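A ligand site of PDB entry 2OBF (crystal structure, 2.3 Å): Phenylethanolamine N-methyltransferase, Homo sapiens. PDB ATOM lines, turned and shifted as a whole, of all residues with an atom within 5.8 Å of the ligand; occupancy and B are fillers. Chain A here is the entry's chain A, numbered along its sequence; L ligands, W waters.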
ATOM      1  N   TYR A  27     -29.945  30.170  -8.832  1.00  0.00           N
ATOM      2  CA  TYR A  27     -29.252  28.967  -9.298  1.00  0.00           C
ATOM      3  C   TYR A  27     -29.725  28.540 -10.680  1.00  0.00           C
ATOM      4  O   TYR A  27     -29.242  27.555 -11.227  1.00  0.00           O
ATOM      5  CB  TYR A  27     -29.426  27.817  -8.295  1.00  0.00           C
ATOM      6  CG  TYR A  27     -28.367  27.832  -7.228  1.00  0.00           C
ATOM      7  CD1 TYR A  27     -28.672  28.206  -5.917  1.00  0.00           C
ATOM      8  CD2 TYR A  27     -27.038  27.561  -7.543  1.00  0.00           C
ATOM      9  CE1 TYR A  27     -27.684  28.318  -4.952  1.00  0.00           C
ATOM     10  CE2 TYR A  27     -26.034  27.666  -6.587  1.00  0.00           C
ATOM     11  CZ  TYR A  27     -26.367  28.054  -5.296  1.00  0.00           C
ATOM     12  OH  TYR A  27     -25.371  28.227  -4.370  1.00  0.00           O
ATOM     13  N   PHE A  30     -26.971  29.645 -13.085  1.00  0.00           N
ATOM     14  CA  PHE A  30     -25.710  28.982 -12.719  1.00  0.00           C
ATOM     15  C   PHE A  30     -25.068  28.217 -13.879  1.00  0.00           C
ATOM     16  O   PHE A  30     -25.605  27.208 -14.358  1.00  0.00           O
ATOM     17  CB  PHE A  30     -25.982  28.000 -11.561  1.00  0.00           C
ATOM     18  CG  PHE A  30     -24.750  27.341 -10.997  1.00  0.00           C
ATOM     19  CD1 PHE A  30     -24.146  27.831  -9.838  1.00  0.00           C
ATOM     20  CD2 PHE A  30     -24.219  26.210 -11.604  1.00  0.00           C
ATOM     21  CE1 PHE A  30     -23.028  27.202  -9.286  1.00  0.00           C
ATOM     22  CE2 PHE A  30     -23.096  25.565 -11.050  1.00  0.00           C
ATOM     23  CZ  PHE A  30     -22.499  26.058  -9.887  1.00  0.00           C
ATOM     24  N   TYR A  35     -18.382  28.123 -13.317  1.00  0.00           N
ATOM     25  CA  TYR A  35     -18.094  27.743 -11.937  1.00  0.00           C
ATOM     26  C   TYR A  35     -16.745  27.020 -11.862  1.00  0.00           C
ATOM     27  O   TYR A  35     -15.923  27.304 -10.994  1.00  0.00           O
ATOM     28  CB  TYR A  35     -19.187  26.830 -11.392  1.00  0.00           C
ATOM     29  CG  TYR A  35     -18.939  26.374  -9.973  1.00  0.00           C
ATOM     30  CD1 TYR A  35     -19.151  27.240  -8.894  1.00  0.00           C
ATOM     31  CD2 TYR A  35     -18.477  25.077  -9.702  1.00  0.00           C
ATOM     32  CE1 TYR A  35     -18.908  26.817  -7.584  1.00  0.00           C
ATOM     33  CE2 TYR A  35     -18.241  24.650  -8.404  1.00  0.00           C
ATOM     34  CZ  TYR A  35     -18.450  25.522  -7.346  1.00  0.00           C
ATOM     35  OH  TYR A  35     -18.206  25.116  -6.050  1.00  0.00           O
ATOM     36  N   TYR A  40     -11.698  25.740 -10.094  1.00  0.00           N
ATOM     37  CA  TYR A  40     -10.846  24.574 -10.240  1.00  0.00           C
ATOM     38  C   TYR A  40      -9.803  24.636 -11.328  1.00  0.00           C
ATOM     39  O   TYR A  40      -9.148  23.652 -11.615  1.00  0.00           O
ATOM     40  CB  TYR A  40     -11.724  23.329 -10.373  1.00  0.00           C
ATOM     41  CG  TYR A  40     -12.571  23.158  -9.139  1.00  0.00           C
ATOM     42  CD1 TYR A  40     -13.866  23.646  -9.088  1.00  0.00           C
ATOM     43  CD2 TYR A  40     -12.032  22.575  -7.985  1.00  0.00           C
ATOM     44  CE1 TYR A  40     -14.627  23.559  -7.925  1.00  0.00           C
ATOM     45  CE2 TYR A  40     -12.777  22.488  -6.814  1.00  0.00           C
ATOM     46  CZ  TYR A  40     -14.073  22.973  -6.788  1.00  0.00           C
ATOM     47  OH  TYR A  40     -14.814  22.891  -5.639  1.00  0.00           O
ATOM     48  N   ASP A  77     -22.909  11.804  -1.941  1.00  0.00           N
ATOM     49  CA  ASP A  77     -22.275  13.110  -2.075  1.00  0.00           C
ATOM     50  C   ASP A  77     -23.395  14.134  -2.277  1.00  0.00           C
ATOM     51  O   ASP A  77     -24.120  14.097  -3.268  1.00  0.00           O
ATOM     52  CB  ASP A  77     -21.316  13.099  -3.286  1.00  0.00           C
ATOM     53  CG  ASP A  77     -20.576  14.412  -3.456  1.00  0.00           C
ATOM     54  OD1 ASP A  77     -20.167  15.011  -2.443  1.00  0.00           O
ATOM     55  OD2 ASP A  77     -20.393  14.850  -4.612  1.00  0.00           O
ATOM     56  N   ILE A  78     -23.536  15.046  -1.309  1.00  0.00           N
ATOM     57  CA  ILE A  78     -24.567  16.076  -1.319  1.00  0.00           C
ATOM     58  C   ILE A  78     -24.198  17.328  -2.105  1.00  0.00           C
ATOM     59  O   ILE A  78     -23.221  18.006  -1.775  1.00  0.00           O
ATOM     60  CB  ILE A  78     -24.913  16.524   0.127  1.00  0.00           C
ATOM     61  CG1 ILE A  78     -25.061  15.298   1.057  1.00  0.00           C
ATOM     62  CG2 ILE A  78     -26.188  17.361   0.120  1.00  0.00           C
ATOM     63  CD1 ILE A  78     -26.196  14.380   0.705  1.00  0.00           C
ATOM     64  N   GLY A  79     -24.993  17.650  -3.126  1.00  0.00           N
ATOM     65  CA  GLY A  79     -24.755  18.842  -3.923  1.00  0.00           C
ATOM     66  C   GLY A  79     -23.390  18.807  -4.586  1.00  0.00           C
ATOM     67  O   GLY A  79     -22.601  19.744  -4.449  1.00  0.00           O
ATOM     68  N   SER A  80     -23.145  17.743  -5.337  1.00  0.00           N
ATOM     69  CA  SER A  80     -21.886  17.514  -6.034  1.00  0.00           C
ATOM     70  C   SER A  80     -21.541  18.591  -7.040  1.00  0.00           C
ATOM     71  O   SER A  80     -20.364  18.775  -7.367  1.00  0.00           O
ATOM     72  CB  SER A  80     -21.935  16.164  -6.749  1.00  0.00           C
ATOM     73  OG  SER A  80     -22.440  15.145  -5.915  1.00  0.00           O
ATOM     74  N   GLY A  81     -22.557  19.286  -7.547  1.00  0.00           N
ATOM     75  CA  GLY A  81     -22.292  20.283  -8.566  1.00  0.00           C
ATOM     76  C   GLY A  81     -21.664  19.578  -9.760  1.00  0.00           C
ATOM     77  O   GLY A  81     -22.040  18.438 -10.072  1.00  0.00           O
ATOM     78  N   PRO A  82     -20.701  20.202 -10.443  1.00  0.00           N
ATOM     79  CA  PRO A  82     -20.057  19.572 -11.599  1.00  0.00           C
ATOM     80  C   PRO A  82     -18.646  19.114 -11.241  1.00  0.00           C
ATOM     81  O   PRO A  82     -17.766  19.121 -12.104  1.00  0.00           O
ATOM     82  CB  PRO A  82     -20.024  20.694 -12.615  1.00  0.00           C
ATOM     83  CG  PRO A  82     -19.620  21.860 -11.732  1.00  0.00           C
ATOM     84  CD  PRO A  82     -20.414  21.656 -10.437  1.00  0.00           C
ATOM     85  N   THR A  83     -18.413  18.756  -9.986  1.00  0.00           N
ATOM     86  CA  THR A  83     -17.067  18.355  -9.567  1.00  0.00           C
ATOM     87  C   THR A  83     -16.990  16.911  -9.041  1.00  0.00           C
ATOM     88  O   THR A  83     -17.997  16.365  -8.585  1.00  0.00           O
ATOM     89  CB  THR A  83     -16.490  19.342  -8.477  1.00  0.00           C
ATOM     90  OG1 THR A  83     -17.167  19.154  -7.227  1.00  0.00           O
ATOM     91  CG2 THR A  83     -16.677  20.783  -8.905  1.00  0.00           C
ATOM     92  N   TYR A  85     -13.579  15.807  -7.563  1.00  0.00           N
ATOM     93  CA  TYR A  85     -12.404  15.773  -6.695  1.00  0.00           C
ATOM     94  C   TYR A  85     -12.711  15.358  -5.258  1.00  0.00           C
ATOM     95  O   TYR A  85     -11.859  14.781  -4.584  1.00  0.00           O
ATOM     96  CB  TYR A  85     -11.730  17.157  -6.678  1.00  0.00           C
ATOM     97  CG  TYR A  85     -12.474  18.158  -5.829  1.00  0.00           C
ATOM     98  CD1 TYR A  85     -12.236  18.242  -4.459  1.00  0.00           C
ATOM     99  CD2 TYR A  85     -13.487  18.955  -6.374  1.00  0.00           C
ATOM    100  CE1 TYR A  85     -12.995  19.091  -3.644  1.00  0.00           C
ATOM    101  CE2 TYR A  85     -14.254  19.800  -5.571  1.00  0.00           C
ATOM    102  CZ  TYR A  85     -14.010  19.861  -4.215  1.00  0.00           C
ATOM    103  OH  TYR A  85     -14.789  20.653  -3.415  1.00  0.00           O
ATOM    104  N   GLN A  86     -13.919  15.667  -4.790  1.00  0.00           N
ATOM    105  CA  GLN A  86     -14.297  15.347  -3.411  1.00  0.00           C
ATOM    106  C   GLN A  86     -14.537  13.859  -3.178  1.00  0.00           C
ATOM    107  O   GLN A  86     -14.836  13.448  -2.058  1.00  0.00           O
ATOM    108  CB  GLN A  86     -15.556  16.135  -2.991  1.00  0.00           C
ATOM    109  CG  GLN A  86     -16.836  15.755  -3.745  1.00  0.00           C
ATOM    110  CD  GLN A  86     -17.052  16.587  -4.987  1.00  0.00           C
ATOM    111  OE1 GLN A  86     -16.128  17.218  -5.491  1.00  0.00           O
ATOM    112  NE2 GLN A  86     -18.282  16.593  -5.492  1.00  0.00           N
ATOM    113  N   ASP A 101     -27.296  16.610  -6.985  1.00  0.00           N
ATOM    114  CA  ASP A 101     -27.328  18.034  -7.240  1.00  0.00           C
ATOM    115  C   ASP A 101     -28.683  18.544  -7.701  1.00  0.00           C
ATOM    116  O   ASP A 101     -29.418  17.879  -8.442  1.00  0.00           O
ATOM    117  CB  ASP A 101     -26.283  18.491  -8.249  1.00  0.00           C
ATOM    118  CG  ASP A 101     -25.944  19.966  -8.093  1.00  0.00           C
ATOM    119  OD1 ASP A 101     -25.339  20.326  -7.054  1.00  0.00           O
ATOM    120  OD2 ASP A 101     -26.298  20.773  -8.971  1.00  0.00           O
ATOM    121  N   PHE A 102     -28.988  19.744  -7.234  1.00  0.00           N
ATOM    122  CA  PHE A 102     -30.234  20.430  -7.521  1.00  0.00           C
ATOM    123  C   PHE A 102     -30.429  20.699  -9.000  1.00  0.00           C
ATOM    124  O   PHE A 102     -31.477  20.420  -9.559  1.00  0.00           O
ATOM    125  CB  PHE A 102     -30.246  21.751  -6.758  1.00  0.00           C
ATOM    126  CG  PHE A 102     -31.567  22.452  -6.758  1.00  0.00           C
ATOM    127  CD1 PHE A 102     -32.640  21.928  -6.049  1.00  0.00           C
ATOM    128  CD2 PHE A 102     -31.730  23.651  -7.445  1.00  0.00           C
ATOM    129  CE1 PHE A 102     -33.869  22.581  -6.017  1.00  0.00           C
ATOM    130  CE2 PHE A 102     -32.964  24.321  -7.414  1.00  0.00           C
ATOM    131  CZ  PHE A 102     -34.027  23.788  -6.701  1.00  0.00           C
ATOM    132  N   LEU A 103     -29.396  21.258  -9.631  1.00  0.00           N
ATOM    133  CA  LEU A 103     -29.447  21.632 -11.042  1.00  0.00           C
ATOM    134  C   LEU A 103     -29.203  20.537 -12.070  1.00  0.00           C
ATOM    135  O   LEU A 103     -28.196  19.853 -12.036  1.00  0.00           O
ATOM    136  CB  LEU A 103     -28.478  22.781 -11.305  1.00  0.00           C
ATOM    137  CG  LEU A 103     -28.649  24.039 -10.465  1.00  0.00           C
ATOM    138  CD1 LEU A 103     -27.613  25.076 -10.878  1.00  0.00           C
ATOM    139  CD2 LEU A 103     -30.055  24.602 -10.649  1.00  0.00           C
ATOM    140  N   ASN A 106     -25.817  20.554 -13.826  1.00  0.00           N
ATOM    141  CA  ASN A 106     -24.633  20.027 -13.165  1.00  0.00           C
ATOM    142  C   ASN A 106     -24.626  18.508 -13.272  1.00  0.00           C
ATOM    143  O   ASN A 106     -23.586  17.917 -13.536  1.00  0.00           O
ATOM    144  CB  ASN A 106     -24.565  20.447 -11.692  1.00  0.00           C
ATOM    145  CG  ASN A 106     -24.069  21.876 -11.520  1.00  0.00           C
ATOM    146  OD1 ASN A 106     -23.172  22.319 -12.239  1.00  0.00           O
ATOM    147  ND2 ASN A 106     -24.624  22.595 -10.550  1.00  0.00           N
ATOM    148  N   ILE A 157     -31.544  16.558  -6.088  1.00  0.00           N
ATOM    149  CA  ILE A 157     -31.679  16.667  -4.640  1.00  0.00           C
ATOM    150  C   ILE A 157     -31.952  18.105  -4.225  1.00  0.00           C
ATOM    151  O   ILE A 157     -31.644  19.043  -4.971  1.00  0.00           O
ATOM    152  CB  ILE A 157     -30.378  16.155  -3.954  1.00  0.00           C
ATOM    153  CG1 ILE A 157     -30.554  16.104  -2.444  1.00  0.00           C
ATOM    154  CG2 ILE A 157     -29.190  17.042  -4.362  1.00  0.00           C
ATOM    155  CD1 ILE A 157     -29.373  15.491  -1.712  1.00  0.00           C
ATOM    156  N   ASP A 158     -32.548  18.254  -3.044  1.00  0.00           N
ATOM    157  CA  ASP A 158     -32.858  19.569  -2.476  1.00  0.00           C
ATOM    158  C   ASP A 158     -32.707  19.495  -0.972  1.00  0.00           C
ATOM    159  O   ASP A 158     -33.563  18.935  -0.281  1.00  0.00           O
ATOM    160  CB  ASP A 158     -34.302  19.975  -2.808  1.00  0.00           C
ATOM    161  CG  ASP A 158     -34.634  21.379  -2.337  1.00  0.00           C
ATOM    162  OD1 ASP A 158     -34.002  21.847  -1.363  1.00  0.00           O
ATOM    163  OD2 ASP A 158     -35.528  22.016  -2.932  1.00  0.00           O
ATOM    164  N   VAL A 159     -31.618  20.056  -0.465  1.00  0.00           N
ATOM    165  CA  VAL A 159     -31.337  20.042   0.957  1.00  0.00           C
ATOM    166  C   VAL A 159     -32.353  20.833   1.772  1.00  0.00           C
ATOM    167  O   VAL A 159     -32.365  20.771   2.998  1.00  0.00           O
ATOM    168  CB  VAL A 159     -29.930  20.593   1.243  1.00  0.00           C
ATOM    169  CG1 VAL A 159     -28.890  19.602   0.745  1.00  0.00           C
ATOM    170  CG2 VAL A 159     -29.767  21.940   0.564  1.00  0.00           C
ATOM    171  N   HIS A 160     -33.215  21.576   1.074  1.00  0.00           N
ATOM    172  CA  HIS A 160     -34.245  22.369   1.742  1.00  0.00           C
ATOM    173  C   HIS A 160     -35.459  21.507   2.101  1.00  0.00           C
ATOM    174  O   HIS A 160     -36.345  21.949   2.816  1.00  0.00           O
ATOM    175  CB  HIS A 160     -34.694  23.522   0.847  1.00  0.00           C
ATOM    176  CG  HIS A 160     -33.613  24.524   0.578  1.00  0.00           C
ATOM    177  ND1 HIS A 160     -33.564  25.271  -0.569  1.00  0.00           N
ATOM    178  CD2 HIS A 160     -32.563  24.927   1.336  1.00  0.00           C
ATOM    179  CE1 HIS A 160     -32.529  26.086  -0.530  1.00  0.00           C
ATOM    180  NE2 HIS A 160     -31.896  25.892   0.628  1.00  0.00           N
ATOM    181  N   SER A 180     -20.085  16.356   1.528  1.00  0.00           N
ATOM    182  CA  SER A 180     -20.704  17.552   0.971  1.00  0.00           C
ATOM    183  C   SER A 180     -19.694  18.665   0.960  1.00  0.00           C
ATOM    184  O   SER A 180     -19.099  18.985   1.991  1.00  0.00           O
ATOM    185  CB  SER A 180     -21.931  17.970   1.776  1.00  0.00           C
ATOM    186  OG  SER A 180     -22.645  19.004   1.084  1.00  0.00           O
ATOM    187  N   ALA A 181     -19.499  19.276  -0.209  1.00  0.00           N
ATOM    188  CA  ALA A 181     -18.534  20.353  -0.346  1.00  0.00           C
ATOM    189  C   ALA A 181     -19.124  21.617  -0.930  1.00  0.00           C
ATOM    190  O   ALA A 181     -19.675  21.610  -2.034  1.00  0.00           O
ATOM    191  CB  ALA A 181     -17.349  19.887  -1.213  1.00  0.00           C
ATOM    192  N   PHE A 182     -19.015  22.714  -0.183  1.00  0.00           N
ATOM    193  CA  PHE A 182     -19.501  24.016  -0.622  1.00  0.00           C
ATOM    194  C   PHE A 182     -20.995  24.110  -0.938  1.00  0.00           C
ATOM    195  O   PHE A 182     -21.427  25.020  -1.656  1.00  0.00           O
ATOM    196  CB  PHE A 182     -18.696  24.441  -1.856  1.00  0.00           C
ATOM    197  CG  PHE A 182     -17.218  24.568  -1.600  1.00  0.00           C
ATOM    198  CD1 PHE A 182     -16.295  23.816  -2.323  1.00  0.00           C
ATOM    199  CD2 PHE A 182     -16.741  25.493  -0.671  1.00  0.00           C
ATOM    200  CE1 PHE A 182     -14.927  23.972  -2.117  1.00  0.00           C
ATOM    201  CE2 PHE A 182     -15.373  25.649  -0.465  1.00  0.00           C
ATOM    202  CZ  PHE A 182     -14.466  24.897  -1.194  1.00  0.00           C
ATOM    203  N   CYS A 183     -21.801  23.210  -0.391  1.00  0.00           N
ATOM    204  CA  CYS A 183     -23.226  23.254  -0.695  1.00  0.00           C
ATOM    205  C   CYS A 183     -24.090  24.039   0.301  1.00  0.00           C
ATOM    206  O   CYS A 183     -24.555  25.126  -0.004  1.00  0.00           O
ATOM    207  CB  CYS A 183     -23.790  21.842  -0.827  1.00  0.00           C
ATOM    208  SG  CYS A 183     -25.571  21.782  -1.234  1.00  0.00           S
ATOM    209  N   ALA A 186     -23.994  27.725   0.672  1.00  0.00           N
ATOM    210  CA  ALA A 186     -24.282  28.367  -0.609  1.00  0.00           C
ATOM    211  C   ALA A 186     -25.759  28.346  -0.982  1.00  0.00           C
ATOM    212  O   ALA A 186     -26.148  28.946  -1.978  1.00  0.00           O
ATOM    213  CB  ALA A 186     -23.477  27.695  -1.702  1.00  0.00           C
ATOM    214  N   VAL A 187     -26.567  27.640  -0.186  1.00  0.00           N
ATOM    215  CA  VAL A 187     -27.990  27.547  -0.460  1.00  0.00           C
ATOM    216  C   VAL A 187     -28.814  28.025   0.741  1.00  0.00           C
ATOM    217  O   VAL A 187     -30.033  27.868   0.777  1.00  0.00           O
ATOM    218  CB  VAL A 187     -28.392  26.098  -0.808  1.00  0.00           C
ATOM    219  CG1 VAL A 187     -27.535  25.581  -1.934  1.00  0.00           C
ATOM    220  CG2 VAL A 187     -28.249  25.211   0.410  1.00  0.00           C
ATOM    221  N   TYR A 222     -20.702  34.588  -4.506  1.00  0.00           N
ATOM    222  CA  TYR A 222     -19.776  33.979  -5.443  1.00  0.00           C
ATOM    223  C   TYR A 222     -20.465  33.966  -6.784  1.00  0.00           C
ATOM    224  O   TYR A 222     -21.693  33.877  -6.849  1.00  0.00           O
ATOM    225  CB  TYR A 222     -19.373  32.559  -5.013  1.00  0.00           C
ATOM    226  CG  TYR A 222     -20.383  31.480  -5.288  1.00  0.00           C
ATOM    227  CD1 TYR A 222     -20.283  30.695  -6.422  1.00  0.00           C
ATOM    228  CD2 TYR A 222     -21.405  31.206  -4.371  1.00  0.00           C
ATOM    229  CE1 TYR A 222     -21.172  29.646  -6.654  1.00  0.00           C
ATOM    230  CE2 TYR A 222     -22.295  30.164  -4.587  1.00  0.00           C
ATOM    231  CZ  TYR A 222     -22.167  29.388  -5.723  1.00  0.00           C
ATOM    232  OH  TYR A 222     -23.017  28.334  -5.945  1.00  0.00           O
HETATM  233  N1  LIG L   1     -19.883  20.454  -4.421  1.00  0.00           N
HETATM  234  C1  LIG L   1     -19.335  21.205  -5.546  1.00  0.00           C
HETATM  235  C2  LIG L   1     -20.277  22.372  -5.903  1.00  0.00           C
HETATM  236  C3  LIG L   1     -20.564  23.353  -4.764  1.00  0.00           C
HETATM  237  S1  LIG L   1     -21.408  24.835  -5.324  1.00  0.00           S
HETATM  238  C4  LIG L   1     -17.934  21.713  -5.234  1.00  0.00           C
HETATM  239  O1  LIG L   1     -17.438  22.605  -5.950  1.00  0.00           O
HETATM  240  O2  LIG L   1     -17.324  21.207  -4.268  1.00  0.00           O
HETATM  241  C5  LIG L   1     -23.076  24.626  -4.587  1.00  0.00           C
HETATM  242  C6  LIG L   1     -23.922  23.571  -5.269  1.00  0.00           C
HETATM  243  O3  LIG L   1     -25.189  23.371  -4.586  1.00  0.00           O
HETATM  244  C7  LIG L   1     -24.237  23.770  -6.755  1.00  0.00           C
HETATM  245  O4  LIG L   1     -23.850  22.630  -7.516  1.00  0.00           O
HETATM  246  C8  LIG L   1     -25.746  24.003  -6.754  1.00  0.00           C
HETATM  247  O5  LIG L   1     -26.389  23.602  -7.947  1.00  0.00           O
HETATM  248  C9  LIG L   1     -26.196  23.149  -5.560  1.00  0.00           C
HETATM  249  N2  LIG L   1     -27.505  23.499  -4.994  1.00  0.00           N
HETATM  250  C10 LIG L   1     -28.264  24.699  -5.193  1.00  0.00           C
HETATM  251  N3  LIG L   1     -29.414  24.680  -4.559  1.00  0.00           N
HETATM  252  C11 LIG L   1     -29.411  23.456  -3.925  1.00  0.00           C
HETATM  253  C12 LIG L   1     -30.403  22.895  -3.095  1.00  0.00           C
HETATM  254  N4  LIG L   1     -31.552  23.515  -2.786  1.00  0.00           N
HETATM  255  N5  LIG L   1     -30.162  21.660  -2.578  1.00  0.00           N
HETATM  256  C13 LIG L   1     -28.991  21.040  -2.892  1.00  0.00           C
HETATM  257  N6  LIG L   1     -27.983  21.489  -3.685  1.00  0.00           N
HETATM  258  C14 LIG L   1     -28.266  22.725  -4.167  1.00  0.00           C
HETATM  259  O   HOH W   1     -32.216  26.189  -4.469  1.00  0.00           O
HETATM  260  O   HOH W   2     -20.387  17.913  -2.601  1.00  0.00           O
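An oxygen (O1) of the ligand is in hydrogen-bond range of the side-chain hydroxyl (OH) of Tyr 35, 2.6 Å away.
O1 of the ligand lies within hydrogen-bond range of OH of Tyr 40 (2.7 Å).
The backbone carbonyl oxygen (O) of Ala 181 is in hydrogen-bond range of a nitrogen (N1) of the ligand (2.7 Å).
The side-chain hydroxyl (OH) of Tyr 85 is in hydrogen-bond range of an oxygen (O2) of the ligand, at 2.7 Å.
The side-chain carboxylate (OD1) of Asp 101 sits at hydrogen-bond distance from an oxygen (O4) of the ligand (2.8 Å).
A nitrogen (N1) of the ligand is in hydrogen-bond range of the backbone carbonyl oxygen of Gly 79, at 2.8 Å.
N5 of the ligand sits at hydrogen-bond distance from N of Val 159 (3.0 Å).
An oxygen (O4) of the ligand lies within hydrogen-bond range of the side-chain amide nitrogen of Asn 106, at 3.1 Å.
The backbone carbonyl oxygen of Ser 80 sits close to a nitrogen (N1) of the ligand (3.4 Å).
A nitrogen (N4) of the ligand lies within hydrogen-bond range of the side-chain carboxylate (OD1) of Asp 158, 3.3 Å away.
A nitrogen (N6) of the ligand is in hydrogen-bond range of the side-chain sulfur (SG) of Cys 183, at 3.5 Å.
A ring nitrogen (ND1) of His 160 is in hydrogen-bond range of a nitrogen (N4) of the ligand, at 3.5 Å.
OH of Tyr 85 lies close to OH of Tyr 40 (3.2 Å).
The side-chain carboxylate (OD2) of Asp 101 lies within hydrogen-bond range of the side-chain amide nitrogen (ND2) of Asn 106.
N of Ile 157 is in hydrogen-bond range of O of Asp 101, at 3.4 Å.
The side-chain carboxylate (OD2) of Asp 77 sits at hydrogen-bond distance from the side-chain hydroxyl (OG) of Ser 80 (2.4 Å).
N of His 160 is in hydrogen-bond range of OD1 of Asp 158.
OG1 of Thr 83 lies within hydrogen-bond range of OE1 of Gln 86 (2.8 Å).
The side-chain hydroxyl (OH) of Tyr 27 lies within hydrogen-bond range of the side-chain hydroxyl (OH) of Tyr 222, 2.8 Å away.
The side-chain hydroxyl of Tyr 27 is in hydrogen-bond range of the backbone carbonyl oxygen of Ala 186 (2.6 Å).
O of Phe 182 lies close to S1 of the ligand, at 3.7 Å.
Tyr 27 touches the ligand.
CA of Gly 81 touches O4 of the ligand, at 3.0 Å.
Thr 83 touches the ligand.
Phe 102 touches the ligand (CB to C14, 3.4 Å).
Leu 103 touches the ligand (CG to O5, 3.4 Å).
O of Ile 157 touches N5 of the ligand (3.8 Å).
Val 187 touches the ligand (CG1 to N3, 3.4 Å).
OH of Tyr 222 touches S1 of the ligand (3.9 Å).
Hydrophobic or aromatic side chains that line the ligand: Tyr 27, Tyr 35, Tyr 40, Tyr 85, Phe 102, Leu 103, Val 159, His 160, Ala 181, Phe 182 and Val 187.
Of the 28 residues printed, 21 come within 4 Å of the ligand.
The nearest printed residue that does not touch the ligand is Ala 186 (4.2 Å).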
